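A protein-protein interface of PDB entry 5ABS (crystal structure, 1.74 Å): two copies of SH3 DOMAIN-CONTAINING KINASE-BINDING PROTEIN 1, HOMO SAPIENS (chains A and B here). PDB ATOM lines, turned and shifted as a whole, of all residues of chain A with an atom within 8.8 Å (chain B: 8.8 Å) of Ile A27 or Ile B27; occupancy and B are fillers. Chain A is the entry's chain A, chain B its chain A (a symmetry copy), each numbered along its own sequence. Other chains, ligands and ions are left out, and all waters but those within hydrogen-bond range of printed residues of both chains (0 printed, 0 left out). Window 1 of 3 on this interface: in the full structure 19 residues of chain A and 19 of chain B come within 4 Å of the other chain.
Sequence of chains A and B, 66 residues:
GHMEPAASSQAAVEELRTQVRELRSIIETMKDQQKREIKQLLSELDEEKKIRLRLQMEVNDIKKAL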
ATOM      1  N   GLN A  19     -17.553  26.247  17.585  1.00  0.00           N
ATOM      2  CA  GLN A  19     -17.439  25.440  18.769  1.00  0.00           C
ATOM      3  C   GLN A  19     -16.157  25.704  19.578  1.00  0.00           C
ATOM      4  O   GLN A  19     -16.151  25.663  20.796  1.00  0.00           O
ATOM      5  CB  GLN A  19     -17.501  23.958  18.398  1.00  0.00           C
ATOM      6  CG  GLN A  19     -18.902  23.481  18.000  1.00  0.00           C
ATOM      7  CD  GLN A  19     -18.910  22.036  17.466  1.00  0.00           C
ATOM      8  OE1 GLN A  19     -17.980  21.284  17.683  1.00  0.00           O
ATOM      9  NE2 GLN A  19     -19.944  21.664  16.740  1.00  0.00           N
ATOM     10  N   VAL A  20     -15.075  25.981  18.893  1.00  0.00           N
ATOM     11  CA  VAL A  20     -13.891  26.451  19.550  1.00  0.00           C
ATOM     12  C   VAL A  20     -14.154  27.803  20.255  1.00  0.00           C
ATOM     13  O   VAL A  20     -13.787  27.920  21.408  1.00  0.00           O
ATOM     14  CB  VAL A  20     -12.686  26.519  18.593  1.00  0.00           C
ATOM     15  CG1 VAL A  20     -11.528  27.296  19.211  1.00  0.00           C
ATOM     16  CG2 VAL A  20     -12.247  25.119  18.223  1.00  0.00           C
ATOM     17  N   ARG A  21     -14.719  28.807  19.594  1.00  0.00           N
ATOM     18  CA  ARG A  21     -15.134  30.064  20.293  1.00  0.00           C
ATOM     19  C   ARG A  21     -16.044  29.782  21.506  1.00  0.00           C
ATOM     20  O   ARG A  21     -15.848  30.382  22.560  1.00  0.00           O
ATOM     21  CB  ARG A  21     -15.814  31.106  19.381  1.00  0.00           C
ATOM     22  CG  ARG A  21     -14.969  31.812  18.307  1.00  0.00           C
ATOM     23  CD  ARG A  21     -15.683  33.066  17.701  1.00  0.00           C
ATOM     24  NE  ARG A  21     -17.052  32.829  17.174  1.00  0.00           N
ATOM     25  CZ  ARG A  21     -17.358  32.243  16.003  1.00  0.00           C
ATOM     26  NH1 ARG A  21     -16.413  31.818  15.150  1.00  0.00           N
ATOM     27  NH2 ARG A  21     -18.651  32.061  15.678  1.00  0.00           N
ATOM     28  N   GLU A  22     -16.965  28.823  21.412  1.00  0.00           N
ATOM     29  CA  GLU A  22     -17.844  28.474  22.540  1.00  0.00           C
ATOM     30  C   GLU A  22     -17.093  27.764  23.690  1.00  0.00           C
ATOM     31  O   GLU A  22     -17.288  28.067  24.891  1.00  0.00           O
ATOM     32  CB  GLU A  22     -19.081  27.658  22.039  1.00  0.00           C
ATOM     33  CG  GLU A  22     -20.191  28.510  21.387  1.00  0.00           C
ATOM     34  CD  GLU A  22     -21.203  27.739  20.457  1.00  0.00           C
ATOM     35  OE1 GLU A  22     -20.966  26.557  20.046  1.00  0.00           O
ATOM     36  OE2 GLU A  22     -22.263  28.343  20.098  1.00  0.00           O
ATOM     37  N   LEU A  23     -16.177  26.859  23.372  1.00  0.00           N
ATOM     38  CA  LEU A  23     -15.404  26.237  24.417  1.00  0.00           C
ATOM     39  C   LEU A  23     -14.469  27.239  25.148  1.00  0.00           C
ATOM     40  O   LEU A  23     -14.338  27.109  26.346  1.00  0.00           O
ATOM     41  CB  LEU A  23     -14.600  25.046  23.971  1.00  0.00           C
ATOM     42  CG  LEU A  23     -15.336  23.778  23.533  1.00  0.00           C
ATOM     43  CD1 LEU A  23     -14.281  22.729  23.245  1.00  0.00           C
ATOM     44  CD2 LEU A  23     -16.355  23.277  24.543  1.00  0.00           C
ATOM     45  N   ARG A  24     -13.881  28.203  24.439  1.00  0.00           N
ATOM     46  CA  ARG A  24     -13.106  29.279  25.061  1.00  0.00           C
ATOM     47  C   ARG A  24     -13.964  30.014  26.105  1.00  0.00           C
ATOM     48  O   ARG A  24     -13.492  30.347  27.170  1.00  0.00           O
ATOM     49  CB  ARG A  24     -12.669  30.302  24.047  1.00  0.00           C
ATOM     50  CG  ARG A  24     -11.419  29.970  23.277  1.00  0.00           C
ATOM     51  CD  ARG A  24     -10.997  31.161  22.407  1.00  0.00           C
ATOM     52  NE  ARG A  24     -10.086  30.683  21.380  1.00  0.00           N
ATOM     53  CZ  ARG A  24      -8.822  30.311  21.608  1.00  0.00           C
ATOM     54  NH1 ARG A  24      -8.260  30.431  22.832  1.00  0.00           N
ATOM     55  NH2 ARG A  24      -8.102  29.847  20.592  1.00  0.00           N
ATOM     56  N   SER A  25     -15.230  30.230  25.795  1.00  0.00           N
ATOM     57  CA  SER A  25     -16.149  30.912  26.714  1.00  0.00           C
ATOM     58  C   SER A  25     -16.516  30.129  27.925  1.00  0.00           C
ATOM     59  O   SER A  25     -16.578  30.675  28.999  1.00  0.00           O
ATOM     60  CB  SER A  25     -17.402  31.351  25.989  1.00  0.00           C
ATOM     61  OG  SER A  25     -17.088  32.566  25.397  1.00  0.00           O
ATOM     62  N   ILE A  26     -16.699  28.841  27.769  1.00  0.00           N
ATOM     63  CA  ILE A  26     -17.032  27.956  28.839  1.00  0.00           C
ATOM     64  C   ILE A  26     -15.890  27.822  29.838  1.00  0.00           C
ATOM     65  O   ILE A  26     -16.116  27.848  31.032  1.00  0.00           O
ATOM     66  CB  ILE A  26     -17.425  26.555  28.278  1.00  0.00           C
ATOM     67  CG1 ILE A  26     -18.760  26.604  27.488  1.00  0.00           C
ATOM     68  CG2 ILE A  26     -17.473  25.500  29.361  1.00  0.00           C
ATOM     69  CD1 ILE A  26     -19.863  27.467  28.073  1.00  0.00           C
ATOM     70  N   ILE A  27     -14.692  27.626  29.322  1.00  0.00           N
ATOM     71  CA  ILE A  27     -13.469  27.607  30.083  1.00  0.00           C
ATOM     72  C   ILE A  27     -13.352  28.868  30.950  1.00  0.00           C
ATOM     73  O   ILE A  27     -13.147  28.721  32.156  1.00  0.00           O
ATOM     74  CB  ILE A  27     -12.246  27.508  29.150  1.00  0.00           C
ATOM     75  CG1 ILE A  27     -12.174  26.110  28.505  1.00  0.00           C
ATOM     76  CG2 ILE A  27     -10.913  27.710  29.889  1.00  0.00           C
ATOM     77  CD1 ILE A  27     -11.219  26.037  27.319  1.00  0.00           C
ATOM     78  N   GLU A  28     -13.504  30.057  30.351  1.00  0.00           N
ATOM     79  CA  GLU A  28     -13.392  31.328  31.119  1.00  0.00           C
ATOM     80  C   GLU A  28     -14.460  31.442  32.207  1.00  0.00           C
ATOM     81  O   GLU A  28     -14.176  31.809  33.351  1.00  0.00           O
ATOM     82  CB  GLU A  28     -13.460  32.530  30.188  1.00  0.00           C
ATOM     83  CG  GLU A  28     -13.346  33.926  30.855  1.00  0.00           C
ATOM     84  CD  GLU A  28     -11.980  34.203  31.535  1.00  0.00           C
ATOM     85  OE1 GLU A  28     -11.027  33.443  31.267  1.00  0.00           O
ATOM     86  OE2 GLU A  28     -11.876  35.120  32.422  1.00  0.00           O
ATOM     87  N   THR A  29     -15.707  31.161  31.851  1.00  0.00           N
ATOM     88  CA  THR A  29     -16.824  31.199  32.802  1.00  0.00           C
ATOM     89  C   THR A  29     -16.647  30.330  34.020  1.00  0.00           C
ATOM     90  O   THR A  29     -16.784  30.802  35.158  1.00  0.00           O
ATOM     91  CB  THR A  29     -18.133  30.799  32.097  1.00  0.00           C
ATOM     92  OG1 THR A  29     -18.385  31.821  31.168  1.00  0.00           O
ATOM     93  CG2 THR A  29     -19.356  30.734  33.084  1.00  0.00           C
ATOM     94  N   MET A  30     -16.315  29.063  33.812  1.00  0.00           N
ATOM     95  CA  MET A  30     -16.183  28.135  34.918  1.00  0.00           C
ATOM     96  C   MET A  30     -14.909  28.347  35.708  1.00  0.00           C
ATOM     97  O   MET A  30     -14.848  27.924  36.839  1.00  0.00           O
ATOM     98  CB  MET A  30     -16.455  26.730  34.372  1.00  0.00           C
ATOM     99  CG  MET A  30     -17.644  26.790  33.391  1.00  0.00           C
ATOM    100  SD  MET A  30     -19.461  26.754  34.173  1.00  0.00           S
ATOM    101  CE  MET A  30     -20.465  27.449  32.617  1.00  0.00           C
ATOM    102  N   LYS A  31     -13.897  29.010  35.145  1.00  0.00           N
ATOM    103  CA  LYS A  31     -12.744  29.514  35.915  1.00  0.00           C
ATOM    104  C   LYS A  31     -13.149  30.662  36.864  1.00  0.00           C
ATOM    105  O   LYS A  31     -12.737  30.724  38.024  1.00  0.00           O
ATOM    106  CB  LYS A  31     -11.634  30.020  34.998  1.00  0.00           C
ATOM    107  CG  LYS A  31     -10.664  31.009  35.668  1.00  0.00           C
ATOM    108  CD  LYS A  31      -9.462  31.397  34.828  1.00  0.00           C
ATOM    109  CE  LYS A  31      -9.760  32.526  33.866  1.00  0.00           C
ATOM    110  NZ  LYS A  31      -9.992  33.871  34.504  1.00  0.00           N
ATOM    111  N   ASP A  32     -13.948  31.583  36.352  1.00  0.00           N
ATOM    112  CA  ASP A  32     -14.436  32.670  37.169  1.00  0.00           C
ATOM    113  C   ASP A  32     -15.351  32.218  38.308  1.00  0.00           C
ATOM    114  O   ASP A  32     -15.280  32.742  39.396  1.00  0.00           O
ATOM    115  CB  ASP A  32     -15.143  33.688  36.277  1.00  0.00           C
ATOM    116  CG  ASP A  32     -14.186  34.457  35.427  1.00  0.00           C
ATOM    117  OD1 ASP A  32     -12.940  34.589  35.745  1.00  0.00           O
ATOM    118  OD2 ASP A  32     -14.688  34.946  34.402  1.00  0.00           O
ATOM    119  N   GLN A  33     -16.203  31.243  38.044  1.00  0.00           N
ATOM    120  CA  GLN A  33     -17.093  30.729  39.024  1.00  0.00           C
ATOM    121  C   GLN A  33     -16.346  29.988  40.143  1.00  0.00           C
ATOM    122  O   GLN A  33     -16.677  30.140  41.340  1.00  0.00           O
ATOM    123  CB  GLN A  33     -18.161  29.829  38.363  1.00  0.00           C
ATOM    124  CG  GLN A  33     -19.189  29.289  39.370  1.00  0.00           C
ATOM    125  CD  GLN A  33     -19.865  30.355  40.272  1.00  0.00           C
ATOM    126  OE1 GLN A  33     -20.626  31.202  39.766  1.00  0.00           O
ATOM    127  NE2 GLN A  33     -19.599  30.317  41.623  1.00  0.00           N
ATOM    128  N   GLN A  34     -15.323  29.231  39.748  1.00  0.00           N
ATOM    129  CA  GLN A  34     -14.448  28.586  40.657  1.00  0.00           C
ATOM    130  C   GLN A  34     -13.643  29.602  41.480  1.00  0.00           C
ATOM    131  O   GLN A  34     -13.484  29.404  42.691  1.00  0.00           O
ATOM    132  CB  GLN A  34     -13.475  27.636  39.904  1.00  0.00           C
ATOM    133  N   GLN B  19      -5.283  25.453  17.447  1.00  0.00           N
ATOM    134  CA  GLN B  19      -6.130  25.980  18.482  1.00  0.00           C
ATOM    135  C   GLN B  19      -6.607  24.921  19.492  1.00  0.00           C
ATOM    136  O   GLN B  19      -6.743  25.183  20.675  1.00  0.00           O
ATOM    137  CB  GLN B  19      -7.349  26.664  17.861  1.00  0.00           C
ATOM    138  CG  GLN B  19      -7.029  28.009  17.199  1.00  0.00           C
ATOM    139  CD  GLN B  19      -8.228  28.596  16.433  1.00  0.00           C
ATOM    140  OE1 GLN B  19      -9.359  28.202  16.644  1.00  0.00           O
ATOM    141  NE2 GLN B  19      -7.974  29.511  15.519  1.00  0.00           N
ATOM    142  N   VAL B  20      -6.854  23.724  19.018  1.00  0.00           N
ATOM    143  CA  VAL B  20      -7.093  22.620  19.901  1.00  0.00           C
ATOM    144  C   VAL B  20      -5.851  22.344  20.783  1.00  0.00           C
ATOM    145  O   VAL B  20      -6.025  22.208  21.978  1.00  0.00           O
ATOM    146  CB  VAL B  20      -7.560  21.363  19.144  1.00  0.00           C
ATOM    147  CG1 VAL B  20      -7.517  20.128  20.037  1.00  0.00           C
ATOM    148  CG2 VAL B  20      -8.957  21.580  18.605  1.00  0.00           C
ATOM    149  N   ARG B  21      -4.650  22.216  20.230  1.00  0.00           N
ATOM    150  CA  ARG B  21      -3.414  22.113  21.068  1.00  0.00           C
ATOM    151  C   ARG B  21      -3.299  23.272  22.080  1.00  0.00           C
ATOM    152  O   ARG B  21      -2.965  23.032  23.237  1.00  0.00           O
ATOM    153  CB  ARG B  21      -2.103  22.013  20.262  1.00  0.00           C
ATOM    154  CG  ARG B  21      -1.831  20.737  19.449  1.00  0.00           C
ATOM    155  CD  ARG B  21      -0.344  20.627  18.972  1.00  0.00           C
ATOM    156  NE  ARG B  21       0.177  21.804  18.230  1.00  0.00           N
ATOM    157  CZ  ARG B  21      -0.081  22.108  16.947  1.00  0.00           C
ATOM    158  NH1 ARG B  21      -0.852  21.329  16.172  1.00  0.00           N
ATOM    159  NH2 ARG B  21       0.433  23.234  16.422  1.00  0.00           N
ATOM    160  N   GLU B  22      -3.660  24.498  21.700  1.00  0.00           N
ATOM    161  CA  GLU B  22      -3.611  25.645  22.622  1.00  0.00           C
ATOM    162  C   GLU B  22      -4.690  25.574  23.726  1.00  0.00           C
ATOM    163  O   GLU B  22      -4.427  25.839  24.923  1.00  0.00           O
ATOM    164  CB  GLU B  22      -3.658  26.990  21.825  1.00  0.00           C
ATOM    165  CG  GLU B  22      -2.316  27.401  21.181  1.00  0.00           C
ATOM    166  CD  GLU B  22      -2.402  28.446  20.004  1.00  0.00           C
ATOM    167  OE1 GLU B  22      -3.507  28.723  19.435  1.00  0.00           O
ATOM    168  OE2 GLU B  22      -1.323  28.992  19.611  1.00  0.00           O
ATOM    169  N   LEU B  23      -5.904  25.156  23.388  1.00  0.00           N
ATOM    170  CA  LEU B  23      -6.910  25.004  24.409  1.00  0.00           C
ATOM    171  C   LEU B  23      -6.570  23.874  25.419  1.00  0.00           C
ATOM    172  O   LEU B  23      -6.844  24.067  26.585  1.00  0.00           O
ATOM    173  CB  LEU B  23      -8.303  24.793  23.881  1.00  0.00           C
ATOM    174  CG  LEU B  23      -8.995  25.938  23.138  1.00  0.00           C
ATOM    175  CD1 LEU B  23     -10.403  25.476  22.824  1.00  0.00           C
ATOM    176  CD2 LEU B  23      -8.998  27.254  23.899  1.00  0.00           C
ATOM    177  N   ARG B  24      -5.976  22.768  24.971  1.00  0.00           N
ATOM    178  CA  ARG B  24      -5.485  21.718  25.867  1.00  0.00           C
ATOM    179  C   ARG B  24      -4.505  22.313  26.893  1.00  0.00           C
ATOM    180  O   ARG B  24      -4.539  21.967  28.053  1.00  0.00           O
ATOM    181  CB  ARG B  24      -4.740  20.652  25.110  1.00  0.00           C
ATOM    182  CG  ARG B  24      -5.589  19.585  24.473  1.00  0.00           C
ATOM    183  CD  ARG B  24      -4.702  18.480  23.884  1.00  0.00           C
ATOM    184  NE  ARG B  24      -5.488  17.720  22.925  1.00  0.00           N
ATOM    185  CZ  ARG B  24      -6.458  16.862  23.258  1.00  0.00           C
ATOM    186  NH1 ARG B  24      -6.733  16.572  24.550  1.00  0.00           N
ATOM    187  NH2 ARG B  24      -7.137  16.261  22.286  1.00  0.00           N
ATOM    188  N   SER B  25      -3.661  23.231  26.453  1.00  0.00           N
ATOM    189  CA  SER B  25      -2.687  23.878  27.340  1.00  0.00           C
ATOM    190  C   SER B  25      -3.277  24.811  28.340  1.00  0.00           C
ATOM    191  O   SER B  25      -2.860  24.821  29.471  1.00  0.00           O
ATOM    192  CB  SER B  25      -1.626  24.594  26.536  1.00  0.00           C
ATOM    193  OG  SER B  25      -0.688  23.627  26.207  1.00  0.00           O
ATOM    194  N   ILE B  26      -4.284  25.549  27.943  1.00  0.00           N
ATOM    195  CA  ILE B  26      -4.966  26.474  28.793  1.00  0.00           C
ATOM    196  C   ILE B  26      -5.731  25.762  29.901  1.00  0.00           C
ATOM    197  O   ILE B  26      -5.692  26.185  31.040  1.00  0.00           O
ATOM    198  CB  ILE B  26      -5.933  27.363  27.954  1.00  0.00           C
ATOM    199  CG1 ILE B  26      -5.161  28.322  27.008  1.00  0.00           C
ATOM    200  CG2 ILE B  26      -6.906  28.127  28.826  1.00  0.00           C
ATOM    201  CD1 ILE B  26      -3.913  28.973  27.574  1.00  0.00           C
ATOM    202  N   ILE B  27      -6.458  24.726  29.529  1.00  0.00           N
ATOM    203  CA  ILE B  27      -7.146  23.844  30.435  1.00  0.00           C
ATOM    204  C   ILE B  27      -6.186  23.318  31.511  1.00  0.00           C
ATOM    205  O   ILE B  27      -6.511  23.457  32.691  1.00  0.00           O
ATOM    206  CB  ILE B  27      -7.768  22.655  29.675  1.00  0.00           C
ATOM    207  CG1 ILE B  27      -8.959  23.130  28.819  1.00  0.00           C
ATOM    208  CG2 ILE B  27      -8.318  21.569  30.613  1.00  0.00           C
ATOM    209  CD1 ILE B  27      -9.404  22.107  27.779  1.00  0.00           C
ATOM    210  N   GLU B  28      -5.036  22.760  31.107  1.00  0.00           N
ATOM    211  CA  GLU B  28      -4.057  22.215  32.087  1.00  0.00           C
ATOM    212  C   GLU B  28      -3.512  23.294  33.022  1.00  0.00           C
ATOM    213  O   GLU B  28      -3.429  23.109  34.240  1.00  0.00           O
ATOM    214  CB  GLU B  28      -2.913  21.511  31.373  1.00  0.00           C
ATOM    215  CG  GLU B  28      -1.818  20.884  32.276  1.00  0.00           C
ATOM    216  CD  GLU B  28      -2.315  19.721  33.173  1.00  0.00           C
ATOM    217  OE1 GLU B  28      -3.425  19.214  32.914  1.00  0.00           O
ATOM    218  OE2 GLU B  28      -1.647  19.375  34.209  1.00  0.00           O
ATOM    219  N   THR B  29      -3.103  24.422  32.457  1.00  0.00           N
ATOM    220  CA  THR B  29      -2.588  25.553  33.238  1.00  0.00           C
ATOM    221  C   THR B  29      -3.524  26.062  34.304  1.00  0.00           C
ATOM    222  O   THR B  29      -3.138  26.186  35.476  1.00  0.00           O
ATOM    223  CB  THR B  29      -2.223  26.720  32.304  1.00  0.00           C
ATOM    224  OG1 THR B  29      -1.142  26.261  31.535  1.00  0.00           O
ATOM    225  CG2 THR B  29      -1.748  27.998  33.088  1.00  0.00           C
ATOM    226  N   MET B  30      -4.766  26.340  33.932  1.00  0.00           N
ATOM    227  CA  MET B  30      -5.720  26.895  34.872  1.00  0.00           C
ATOM    228  C   MET B  30      -6.237  25.863  35.853  1.00  0.00           C
ATOM    229  O   MET B  30      -6.723  26.242  36.894  1.00  0.00           O
ATOM    230  CB  MET B  30      -6.754  27.686  34.064  1.00  0.00           C
ATOM    231  CG  MET B  30      -6.030  28.475  32.954  1.00  0.00           C
ATOM    232  SD  MET B  30      -5.215  30.205  33.462  1.00  0.00           S
ATOM    233  CE  MET B  30      -3.990  30.418  31.924  1.00  0.00           C
ATOM    234  N   LYS B  31      -6.126  24.567  35.555  1.00  0.00           N
ATOM    235  CA  LYS B  31      -6.329  23.497  36.549  1.00  0.00           C
ATOM    236  C   LYS B  31      -5.211  23.489  37.615  1.00  0.00           C
ATOM    237  O   LYS B  31      -5.456  23.342  38.813  1.00  0.00           O
ATOM    238  CB  LYS B  31      -6.373  22.120  35.892  1.00  0.00           C
ATOM    239  CG  LYS B  31      -6.057  20.955  36.847  1.00  0.00           C
ATOM    240  CD  LYS B  31      -6.256  19.571  36.257  1.00  0.00           C
ATOM    241  CE  LYS B  31      -5.056  19.093  35.468  1.00  0.00           C
ATOM    242  NZ  LYS B  31      -3.832  18.780  36.287  1.00  0.00           N
ATOM    243  N   ASP B  32      -3.976  23.629  37.162  1.00  0.00           N
ATOM    244  CA  ASP B  32      -2.860  23.694  38.077  1.00  0.00           C
ATOM    245  C   ASP B  32      -2.885  24.924  38.987  1.00  0.00           C
ATOM    246  O   ASP B  32      -2.555  24.834  40.147  1.00  0.00           O
ATOM    247  CB  ASP B  32      -1.558  23.634  37.282  1.00  0.00           C
ATOM    248  CG  ASP B  32      -1.305  22.275  36.713  1.00  0.00           C
ATOM    249  OD1 ASP B  32      -1.838  21.211  37.217  1.00  0.00           O
ATOM    250  OD2 ASP B  32      -0.550  22.264  35.727  1.00  0.00           O
ATOM    251  N   GLN B  33      -3.279  26.064  38.447  1.00  0.00           N
ATOM    252  CA  GLN B  33      -3.356  27.268  39.194  1.00  0.00           C
ATOM    253  C   GLN B  33      -4.457  27.209  40.263  1.00  0.00           C
ATOM    254  O   GLN B  33      -4.256  27.662  41.412  1.00  0.00           O
ATOM    255  CB  GLN B  33      -3.546  28.477  38.251  1.00  0.00           C
ATOM    256  CG  GLN B  33      -3.579  29.818  39.001  1.00  0.00           C
ATOM    257  CD  GLN B  33      -2.393  30.071  39.970  1.00  0.00           C
ATOM    258  OE1 GLN B  33      -1.242  30.215  39.516  1.00  0.00           O
ATOM    259  NE2 GLN B  33      -2.666  30.135  41.318  1.00  0.00           N
ATOM    260  N   GLN B  34      -5.590  26.615  39.889  1.00  0.00           N
ATOM    261  CA  GLN B  34      -6.656  26.358  40.787  1.00  0.00           C
ATOM    262  C   GLN B  34      -6.247  25.352  41.873  1.00  0.00           C
ATOM    263  O   GLN B  34      -6.593  25.556  43.043  1.00  0.00           O
ATOM    264  CB  GLN B  34      -7.901  25.825  40.024  1.00  0.00           C
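Among the printed residues, merely in contact across the chains: Arg A24 with Leu B23, Val A20 with Gln B19 and Ile A27 with Ile B27.
Of the printed residues of chain B, Val A20 touches Gln B19 (3.5 Å).
Of the printed residues of chain B, Ile A27 touches Ile B27 (3.98 Å).
Asp A32 touches none of the printed residues of chain B.
Of the printed residues of chain A, Gln B19 touches Val A20.
Ile B27 touches one residue of chain A.
The nearest printed residue of chain A that does not touch Leu B23 is Val A20 (4.2 Å).
Of the 16 printed residues of chain A, 3 touch a printed residue of chain B.
Along chain A the printed residues that touch a printed residue of chain B span positions 20 to 27.
Hydrophobic or aromatic side chains of chain B that line the printed part of chain A: Leu B23 and Ile B27.
Among the printed residues, 3 pairs touch across the chains.
Among the printed residues, no Asp or Glu carboxylate lies within 4 Å of a Lys or Arg side-chain nitrogen of the other chain.
Val A20 touches Gln B19, but with the chains exchanged Gln A19 does not touch Val B20 (8.4 Å).
Arg A24 touches Leu B23, but with the chains exchanged Leu A23 does not touch Arg B24 (8.5 Å).
Ile B27 touches its own counterpart, Ile A27.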
